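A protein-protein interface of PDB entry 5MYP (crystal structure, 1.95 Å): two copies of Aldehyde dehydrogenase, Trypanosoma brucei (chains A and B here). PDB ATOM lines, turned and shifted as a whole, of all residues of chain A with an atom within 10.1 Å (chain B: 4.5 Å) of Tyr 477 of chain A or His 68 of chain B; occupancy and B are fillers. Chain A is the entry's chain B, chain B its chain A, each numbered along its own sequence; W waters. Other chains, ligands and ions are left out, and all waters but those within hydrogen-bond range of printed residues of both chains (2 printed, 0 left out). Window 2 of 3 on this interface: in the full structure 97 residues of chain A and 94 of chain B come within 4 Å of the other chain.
OE1 of Glu 71 of chain B is in hydrogen-bond range of OH of Tyr 477 of chain A (2.6 Å).
The side-chain hydroxyl of Ser 482 of chain A lies within hydrogen-bond range of the side-chain carboxylate of Asp 70 of chain B (2.8 Å).
The guanidinium group (NH2) of Arg 69 of chain B is in hydrogen-bond range of the side-chain amide oxygen (OD1) of Asn 486 of chain A, at 2.9 Å.
Water W1 lies within hydrogen-bond range of the backbone carbonyl oxygen (O) of Tyr 477 of chain A (2.6 Å) and the side-chain carboxylate (OD2) of Asp 312 of chain B (2.7 Å).
Water W2 bridges the side-chain carboxylate of Asp 312 of chain B (2.7 Å) and the backbone NH of Tyr 477 of chain A (2.9 Å).
The backbone carbonyl oxygen (O) of His 68 of chain B lies within hydrogen-bond range of the side-chain hydroxyl (OG1) of Thr 72 of chain B.
The side-chain hydroxyl (OG) of Ser 482 of chain A lies within hydrogen-bond range of the backbone carbonyl oxygen (O) of Thr 478 of chain A (3.2 Å).
OG1 of Thr 478 of chain A is in hydrogen-bond range of N of Lys 481 of chain A, at 3.2 Å.
The side-chain amino group (NZ) of Lys 481 of chain A is in hydrogen-bond range of the backbone carbonyl oxygen (O) of Phe 474 of chain A (2.6 Å).
O of Ser 482 of chain A lies close to ND2 of Asn 486 of chain A, at 3.3 Å.
A ring nitrogen (ND1) of His 68 of chain B is in hydrogen-bond range of the backbone NH (N) of Asp 70 of chain B (3.2 Å).
No position is printed for both chains.
Of the 7 pairs that touch across the chains among the printed residues, none has its exchanged pair printed and touching as well.
Arg 473 of chain A touches none of the printed residues of chain B.
Printed residues of chain B within 4 Å of Tyr 477 of chain A: His 68, Asp 70 and Glu 71.
Of the printed residues of chain B, Lys 481 of chain A touches Asp 70 (3.9 Å).
Of the printed residues of chain B, Leu 485 of chain A touches Asp 70.
Of the printed residues of chain B, Asn 486 of chain A touches Arg 69 (2.9 Å).
His 68 of chain B touches just one residue of chain A: Tyr 477.
Printed residues of chain A within 4 Å of Arg 69 of chain B: Asn 486 (2.9 Å).
Asp 70 of chain B touches just these residues of chain A: Tyr 477 (3.7 Å), Lys 481 (3.9 Å), Ser 482 (2.8 Å) and Leu 485 (3.5 Å).
Glu 71 of chain B touches just one residue of chain A: Tyr 477 (2.6 Å).
The nearest residue of chain A that does not touch His 68 of chain B is Ser 482 of chain A (4.6 Å).
The nearest printed residue of chain B that does not touch Lys 481 of chain A is Glu 71 of chain B (6.3 Å).
Hydrophobic or aromatic side chains of chain A that line the printed part of chain B: Tyr 477 and Leu 485.
Among the printed residues, 7 pairs touch across the chains.
Among the printed residues, no Asp or Glu carboxylate lies within 4 Å of a Lys or Arg side-chain nitrogen of the other chain.
Among the printed residues, pairs that only touch across the chains: Tyr 477 of chain A with His 68 of chain B (3.6 Å), Tyr 477 of chain A with Asp 70 of chain B (3.7 Å), Lys 481 of chain A with Asp 70 of chain B (3.9 Å) and Leu 485 of chain A with Asp 70 of chain B (3.5 Å).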
ATOM      1  N   ILE A 469      20.457 -13.075 -19.329  1.00  0.00           N
ATOM      2  CA  ILE A 469      20.173 -12.243 -18.141  1.00  0.00           C
ATOM      3  C   ILE A 469      20.573 -12.922 -16.822  1.00  0.00           C
ATOM      4  O   ILE A 469      21.016 -12.245 -15.891  1.00  0.00           O
ATOM      5  CB  ILE A 469      18.688 -11.785 -18.065  1.00  0.00           C
ATOM      6  CG1 ILE A 469      17.734 -12.980 -17.873  1.00  0.00           C
ATOM      7  CG2 ILE A 469      18.323 -10.954 -19.295  1.00  0.00           C
ATOM      8  CD1 ILE A 469      16.262 -12.634 -17.987  1.00  0.00           C
ATOM      9  N   THR A 471      23.131 -14.754 -16.158  1.00  0.00           N
ATOM     10  CA  THR A 471      24.578 -14.700 -15.899  1.00  0.00           C
ATOM     11  C   THR A 471      24.985 -13.547 -14.972  1.00  0.00           C
ATOM     12  O   THR A 471      26.032 -13.628 -14.325  1.00  0.00           O
ATOM     13  CB  THR A 471      25.405 -14.570 -17.201  1.00  0.00           C
ATOM     14  OG1 THR A 471      25.029 -13.376 -17.898  1.00  0.00           O
ATOM     15  CG2 THR A 471      25.207 -15.779 -18.113  1.00  0.00           C
ATOM     16  N   VAL A 472      24.175 -12.483 -14.919  1.00  0.00           N
ATOM     17  CA  VAL A 472      24.515 -11.275 -14.144  1.00  0.00           C
ATOM     18  C   VAL A 472      23.474 -10.767 -13.127  1.00  0.00           C
ATOM     19  O   VAL A 472      23.862 -10.112 -12.155  1.00  0.00           O
ATOM     20  CB  VAL A 472      24.918 -10.100 -15.076  1.00  0.00           C
ATOM     21  CG1 VAL A 472      26.248 -10.398 -15.759  1.00  0.00           C
ATOM     22  CG2 VAL A 472      23.833  -9.804 -16.109  1.00  0.00           C
ATOM     23  N   ARG A 473      22.183 -11.054 -13.318  1.00  0.00           N
ATOM     24  CA  ARG A 473      21.143 -10.388 -12.511  1.00  0.00           C
ATOM     25  C   ARG A 473      21.112 -10.785 -11.024  1.00  0.00           C
ATOM     26  O   ARG A 473      20.862  -9.929 -10.173  1.00  0.00           O
ATOM     27  CB  ARG A 473      19.742 -10.534 -13.144  1.00  0.00           C
ATOM     28  CG  ARG A 473      19.126 -11.931 -13.138  1.00  0.00           C
ATOM     29  CD  ARG A 473      17.630 -11.872 -13.434  1.00  0.00           C
ATOM     30  NE  ARG A 473      17.123 -13.091 -14.070  1.00  0.00           N
ATOM     31  CZ  ARG A 473      15.834 -13.389 -14.245  1.00  0.00           C
ATOM     32  NH1 ARG A 473      14.877 -12.570 -13.817  1.00  0.00           N
ATOM     33  NH2 ARG A 473      15.498 -14.526 -14.847  1.00  0.00           N
ATOM     34  N   PHE A 474      21.386 -12.051 -10.713  1.00  0.00           N
ATOM     35  CA  PHE A 474      21.179 -12.577  -9.355  1.00  0.00           C
ATOM     36  C   PHE A 474      22.335 -12.258  -8.404  1.00  0.00           C
ATOM     37  O   PHE A 474      23.488 -12.543  -8.725  1.00  0.00           O
ATOM     38  CB  PHE A 474      20.987 -14.099  -9.380  1.00  0.00           C
ATOM     39  CG  PHE A 474      19.771 -14.549 -10.135  1.00  0.00           C
ATOM     40  CD1 PHE A 474      18.504 -14.167  -9.715  1.00  0.00           C
ATOM     41  CD2 PHE A 474      19.884 -15.368 -11.260  1.00  0.00           C
ATOM     42  CE1 PHE A 474      17.368 -14.578 -10.402  1.00  0.00           C
ATOM     43  CE2 PHE A 474      18.754 -15.782 -11.954  1.00  0.00           C
ATOM     44  CZ  PHE A 474      17.493 -15.386 -11.521  1.00  0.00           C
ATOM     45  N   PRO A 475      22.027 -11.692  -7.215  1.00  0.00           N
ATOM     46  CA  PRO A 475      23.014 -11.685  -6.127  1.00  0.00           C
ATOM     47  C   PRO A 475      23.326 -13.127  -5.655  1.00  0.00           C
ATOM     48  O   PRO A 475      22.573 -14.039  -5.995  1.00  0.00           O
ATOM     49  CB  PRO A 475      22.320 -10.881  -5.017  1.00  0.00           C
ATOM     50  CG  PRO A 475      21.212 -10.143  -5.678  1.00  0.00           C
ATOM     51  CD  PRO A 475      20.793 -10.974  -6.847  1.00  0.00           C
ATOM     52  N   PRO A 476      24.384 -13.355  -4.868  1.00  0.00           N
ATOM     53  CA  PRO A 476      25.253 -12.321  -4.297  1.00  0.00           C
ATOM     54  C   PRO A 476      26.215 -11.694  -5.306  1.00  0.00           C
ATOM     55  O   PRO A 476      26.557 -12.312  -6.317  1.00  0.00           O
ATOM     56  CB  PRO A 476      26.024 -13.081  -3.211  1.00  0.00           C
ATOM     57  CG  PRO A 476      26.058 -14.493  -3.677  1.00  0.00           C
ATOM     58  CD  PRO A 476      24.861 -14.716  -4.559  1.00  0.00           C
ATOM     59  N   TYR A 477      26.631 -10.466  -5.015  1.00  0.00           N
ATOM     60  CA  TYR A 477      27.486  -9.697  -5.911  1.00  0.00           C
ATOM     61  C   TYR A 477      28.943 -10.083  -5.684  1.00  0.00           C
ATOM     62  O   TYR A 477      29.626  -9.518  -4.828  1.00  0.00           O
ATOM     63  CB  TYR A 477      27.232  -8.196  -5.730  1.00  0.00           C
ATOM     64  CG  TYR A 477      25.809  -7.827  -6.103  1.00  0.00           C
ATOM     65  CD1 TYR A 477      25.385  -7.890  -7.427  1.00  0.00           C
ATOM     66  CD2 TYR A 477      24.876  -7.455  -5.135  1.00  0.00           C
ATOM     67  CE1 TYR A 477      24.082  -7.579  -7.784  1.00  0.00           C
ATOM     68  CE2 TYR A 477      23.567  -7.139  -5.481  1.00  0.00           C
ATOM     69  CZ  TYR A 477      23.176  -7.201  -6.807  1.00  0.00           C
ATOM     70  OH  TYR A 477      21.887  -6.898  -7.176  1.00  0.00           O
ATOM     71  N   THR A 478      29.391 -11.067  -6.462  1.00  0.00           N
ATOM     72  CA  THR A 478      30.723 -11.645  -6.326  1.00  0.00           C
ATOM     73  C   THR A 478      31.749 -10.897  -7.174  1.00  0.00           C
ATOM     74  O   THR A 478      31.391 -10.102  -8.045  1.00  0.00           O
ATOM     75  CB  THR A 478      30.716 -13.127  -6.752  1.00  0.00           C
ATOM     76  OG1 THR A 478      30.293 -13.238  -8.119  1.00  0.00           O
ATOM     77  CG2 THR A 478      29.774 -13.931  -5.866  1.00  0.00           C
ATOM     78  N   THR A 479      33.028 -11.161  -6.902  1.00  0.00           N
ATOM     79  CA  THR A 479      34.127 -10.627  -7.715  1.00  0.00           C
ATOM     80  C   THR A 479      34.053 -11.138  -9.163  1.00  0.00           C
ATOM     81  O   THR A 479      34.386 -10.404 -10.094  1.00  0.00           O
ATOM     82  CB  THR A 479      35.505 -10.982  -7.111  1.00  0.00           C
ATOM     83  OG1 THR A 479      35.540 -10.608  -5.726  1.00  0.00           O
ATOM     84  CG2 THR A 479      36.632 -10.258  -7.845  1.00  0.00           C
ATOM     85  N   ALA A 480      33.610 -12.387  -9.335  1.00  0.00           N
ATOM     86  CA  ALA A 480      33.379 -12.978 -10.662  1.00  0.00           C
ATOM     87  C   ALA A 480      32.326 -12.223 -11.484  1.00  0.00           C
ATOM     88  O   ALA A 480      32.527 -11.972 -12.679  1.00  0.00           O
ATOM     89  CB  ALA A 480      32.977 -14.440 -10.524  1.00  0.00           C
ATOM     90  N   LYS A 481      31.210 -11.866 -10.845  1.00  0.00           N
ATOM     91  CA  LYS A 481      30.154 -11.088 -11.503  1.00  0.00           C
ATOM     92  C   LYS A 481      30.646  -9.697 -11.909  1.00  0.00           C
ATOM     93  O   LYS A 481      30.354  -9.232 -13.017  1.00  0.00           O
ATOM     94  CB  LYS A 481      28.929 -10.950 -10.594  1.00  0.00           C
ATOM     95  CG  LYS A 481      27.716 -10.331 -11.276  1.00  0.00           C
ATOM     96  CD  LYS A 481      26.693  -9.835 -10.267  1.00  0.00           C
ATOM     97  CE  LYS A 481      26.075 -10.958  -9.441  1.00  0.00           C
ATOM     98  NZ  LYS A 481      25.521 -12.055 -10.276  1.00  0.00           N
ATOM     99  N   SER A 482      31.375  -9.041 -11.005  1.00  0.00           N
ATOM    100  CA  SER A 482      31.973  -7.730 -11.281  1.00  0.00           C
ATOM    101  C   SER A 482      32.882  -7.753 -12.512  1.00  0.00           C
ATOM    102  O   SER A 482      32.823  -6.838 -13.334  1.00  0.00           O
ATOM    103  CB  SER A 482      32.751  -7.229 -10.063  1.00  0.00           C
ATOM    104  OG  SER A 482      31.883  -7.066  -8.957  1.00  0.00           O
ATOM    105  N   ARG A 483      33.700  -8.798 -12.633  1.00  0.00           N
ATOM    106  CA  ARG A 483      34.567  -8.986 -13.801  1.00  0.00           C
ATOM    107  C   ARG A 483      33.774  -9.185 -15.097  1.00  0.00           C
ATOM    108  O   ARG A 483      34.166  -8.669 -16.145  1.00  0.00           O
ATOM    109  CB  ARG A 483      35.511 -10.179 -13.587  1.00  0.00           C
ATOM    110  CG  ARG A 483      36.708  -9.903 -12.688  1.00  0.00           C
ATOM    111  CD  ARG A 483      37.881 -10.813 -13.028  1.00  0.00           C
ATOM    112  NE  ARG A 483      38.834 -10.895 -11.924  1.00  0.00           N
ATOM    113  CZ  ARG A 483      38.657 -11.630 -10.828  1.00  0.00           C
ATOM    114  NH1 ARG A 483      39.587 -11.638  -9.880  1.00  0.00           N
ATOM    115  NH2 ARG A 483      37.558 -12.358 -10.671  1.00  0.00           N
ATOM    116  N   VAL A 484      32.668  -9.926 -15.016  1.00  0.00           N
ATOM    117  CA  VAL A 484      31.780 -10.155 -16.171  1.00  0.00           C
ATOM    118  C   VAL A 484      31.119  -8.844 -16.632  1.00  0.00           C
ATOM    119  O   VAL A 484      31.114  -8.536 -17.831  1.00  0.00           O
ATOM    120  CB  VAL A 484      30.702 -11.230 -15.859  1.00  0.00           C
ATOM    121  CG1 VAL A 484      29.646 -11.316 -16.964  1.00  0.00           C
ATOM    122  CG2 VAL A 484      31.347 -12.597 -15.634  1.00  0.00           C
ATOM    123  N   LEU A 485      30.578  -8.082 -15.681  1.00  0.00           N
ATOM    124  CA  LEU A 485      29.945  -6.794 -15.990  1.00  0.00           C
ATOM    125  C   LEU A 485      30.950  -5.720 -16.435  1.00  0.00           C
ATOM    126  O   LEU A 485      30.653  -4.936 -17.342  1.00  0.00           O
ATOM    127  CB  LEU A 485      29.113  -6.290 -14.803  1.00  0.00           C
ATOM    128  CG  LEU A 485      27.830  -7.088 -14.529  1.00  0.00           C
ATOM    129  CD1 LEU A 485      27.248  -6.720 -13.176  1.00  0.00           C
ATOM    130  CD2 LEU A 485      26.789  -6.896 -15.626  1.00  0.00           C
ATOM    131  N   ASN A 486      32.127  -5.687 -15.805  1.00  0.00           N
ATOM    132  CA  ASN A 486      33.204  -4.766 -16.214  1.00  0.00           C
ATOM    133  C   ASN A 486      33.715  -5.024 -17.637  1.00  0.00           C
ATOM    134  O   ASN A 486      34.160  -4.089 -18.301  1.00  0.00           O
ATOM    135  CB  ASN A 486      34.384  -4.806 -15.225  1.00  0.00           C
ATOM    136  CG  ASN A 486      34.066  -4.130 -13.896  1.00  0.00           C
ATOM    137  OD1 ASN A 486      33.050  -3.447 -13.745  1.00  0.00           O
ATOM    138  ND2 ASN A 486      34.940  -4.329 -12.919  1.00  0.00           N
ATOM    139  N   ARG B  66      22.115   3.088  -1.497  1.00  0.00           N
ATOM    140  CA  ARG B  66      22.922   1.936  -1.018  1.00  0.00           C
ATOM    141  C   ARG B  66      22.810   0.718  -1.953  1.00  0.00           C
ATOM    142  O   ARG B  66      22.871  -0.439  -1.514  1.00  0.00           O
ATOM    143  CB  ARG B  66      22.601   1.565   0.434  1.00  0.00           C
ATOM    144  CG  ARG B  66      23.745   0.834   1.140  1.00  0.00           C
ATOM    145  CD  ARG B  66      23.461   0.636   2.613  1.00  0.00           C
ATOM    146  NE  ARG B  66      22.295  -0.224   2.823  1.00  0.00           N
ATOM    147  CZ  ARG B  66      21.479  -0.192   3.877  1.00  0.00           C
ATOM    148  NH1 ARG B  66      21.658   0.671   4.875  1.00  0.00           N
ATOM    149  NH2 ARG B  66      20.455  -1.040   3.927  1.00  0.00           N
ATOM    150  N   ARG B  67      22.648   1.000  -3.245  1.00  0.00           N
ATOM    151  CA  ARG B  67      22.522  -0.021  -4.267  1.00  0.00           C
ATOM    152  C   ARG B  67      23.930  -0.374  -4.744  1.00  0.00           C
ATOM    153  O   ARG B  67      24.753   0.520  -4.974  1.00  0.00           O
ATOM    154  CB  ARG B  67      21.648   0.516  -5.403  1.00  0.00           C
ATOM    155  CG  ARG B  67      21.357  -0.476  -6.510  1.00  0.00           C
ATOM    156  CD  ARG B  67      19.893  -0.455  -6.941  1.00  0.00           C
ATOM    157  NE  ARG B  67      19.298   0.873  -7.104  1.00  0.00           N
ATOM    158  CZ  ARG B  67      19.541   1.694  -8.119  1.00  0.00           C
ATOM    159  NH1 ARG B  67      20.410   1.356  -9.057  1.00  0.00           N
ATOM    160  NH2 ARG B  67      18.928   2.868  -8.182  1.00  0.00           N
ATOM    161  N   HIS B  68      24.209  -1.672  -4.868  1.00  0.00           N
ATOM    162  CA  HIS B  68      25.532  -2.155  -5.295  1.00  0.00           C
ATOM    163  C   HIS B  68      25.799  -1.766  -6.752  1.00  0.00           C
ATOM    164  O   HIS B  68      24.871  -1.730  -7.565  1.00  0.00           O
ATOM    165  CB  HIS B  68      25.619  -3.679  -5.132  1.00  0.00           C
ATOM    166  CG  HIS B  68      27.013  -4.225  -5.202  1.00  0.00           C
ATOM    167  ND1 HIS B  68      27.659  -4.480  -6.394  1.00  0.00           N
ATOM    168  CD2 HIS B  68      27.874  -4.595  -4.225  1.00  0.00           C
ATOM    169  CE1 HIS B  68      28.864  -4.962  -6.148  1.00  0.00           C
ATOM    170  NE2 HIS B  68      29.018  -5.046  -4.839  1.00  0.00           N
ATOM    171  N   ARG B  69      27.063  -1.464  -7.055  1.00  0.00           N
ATOM    172  CA  ARG B  69      27.501  -1.055  -8.399  1.00  0.00           C
ATOM    173  C   ARG B  69      26.975  -1.959  -9.516  1.00  0.00           C
ATOM    174  O   ARG B  69      26.474  -1.480 -10.532  1.00  0.00           O
ATOM    175  CB  ARG B  69      29.032  -1.016  -8.461  1.00  0.00           C
ATOM    176  CG  ARG B  69      29.602  -0.971  -9.867  1.00  0.00           C
ATOM    177  CD  ARG B  69      31.115  -0.989  -9.842  1.00  0.00           C
ATOM    178  NE  ARG B  69      31.653  -1.249 -11.173  1.00  0.00           N
ATOM    179  CZ  ARG B  69      31.951  -0.321 -12.084  1.00  0.00           C
ATOM    180  NH1 ARG B  69      31.781   0.976 -11.834  1.00  0.00           N
ATOM    181  NH2 ARG B  69      32.436  -0.699 -13.264  1.00  0.00           N
ATOM    182  N   ASP B  70      27.127  -3.265  -9.319  1.00  0.00           N
ATOM    183  CA  ASP B  70      26.671  -4.269 -10.287  1.00  0.00           C
ATOM    184  C   ASP B  70      25.155  -4.247 -10.496  1.00  0.00           C
ATOM    185  O   ASP B  70      24.688  -4.448 -11.617  1.00  0.00           O
ATOM    186  CB  ASP B  70      27.113  -5.677  -9.856  1.00  0.00           C
ATOM    187  CG  ASP B  70      28.633  -5.856  -9.871  1.00  0.00           C
ATOM    188  OD1 ASP B  70      29.359  -4.959 -10.350  1.00  0.00           O
ATOM    189  OD2 ASP B  70      29.097  -6.905  -9.385  1.00  0.00           O
ATOM    190  N   GLU B  71      24.396  -4.004  -9.426  1.00  0.00           N
ATOM    191  CA  GLU B  71      22.939  -3.852  -9.535  1.00  0.00           C
ATOM    192  C   GLU B  71      22.595  -2.617 -10.374  1.00  0.00           C
ATOM    193  O   GLU B  71      21.728  -2.675 -11.244  1.00  0.00           O
ATOM    194  CB  GLU B  71      22.284  -3.758  -8.153  1.00  0.00           C
ATOM    195  CG  GLU B  71      20.781  -4.017  -8.170  1.00  0.00           C
ATOM    196  CD  GLU B  71      20.175  -4.126  -6.778  1.00  0.00           C
ATOM    197  OE1 GLU B  71      20.708  -4.891  -5.947  1.00  0.00           O
ATOM    198  OE2 GLU B  71      19.158  -3.453  -6.513  1.00  0.00           O
ATOM    199  N   THR B  72      23.293  -1.514 -10.114  1.00  0.00           N
ATOM    200  CA  THR B  72      23.119  -0.277 -10.880  1.00  0.00           C
ATOM    201  C   THR B  72      23.519  -0.437 -12.349  1.00  0.00           C
ATOM    202  O   THR B  72      22.860   0.119 -13.232  1.00  0.00           O
ATOM    203  CB  THR B  72      23.912   0.883 -10.242  1.00  0.00           C
ATOM    204  OG1 THR B  72      23.456   1.077  -8.900  1.00  0.00           O
ATOM    205  CG2 THR B  72      23.734   2.188 -11.027  1.00  0.00           C
ATOM    206  N   ASP B 312      25.613  -5.072   0.733  1.00  0.00           N
ATOM    207  CA  ASP B 312      25.172  -5.081  -0.666  1.00  0.00           C
ATOM    208  C   ASP B 312      23.654  -4.915  -0.825  1.00  0.00           C
ATOM    209  O   ASP B 312      23.135  -5.043  -1.941  1.00  0.00           O
ATOM    210  CB  ASP B 312      25.592  -6.397  -1.333  1.00  0.00           C
ATOM    211  CG  ASP B 312      27.098  -6.621  -1.318  1.00  0.00           C
ATOM    212  OD1 ASP B 312      27.859  -5.689  -0.983  1.00  0.00           O
ATOM    213  OD2 ASP B 312      27.522  -7.746  -1.650  1.00  0.00           O
HETATM  214  O   HOH W   1      30.015  -8.513  -2.429  1.00  0.00           O
HETATM  215  O   HOH W   2      25.690  -9.586  -2.431  1.00  0.00           O
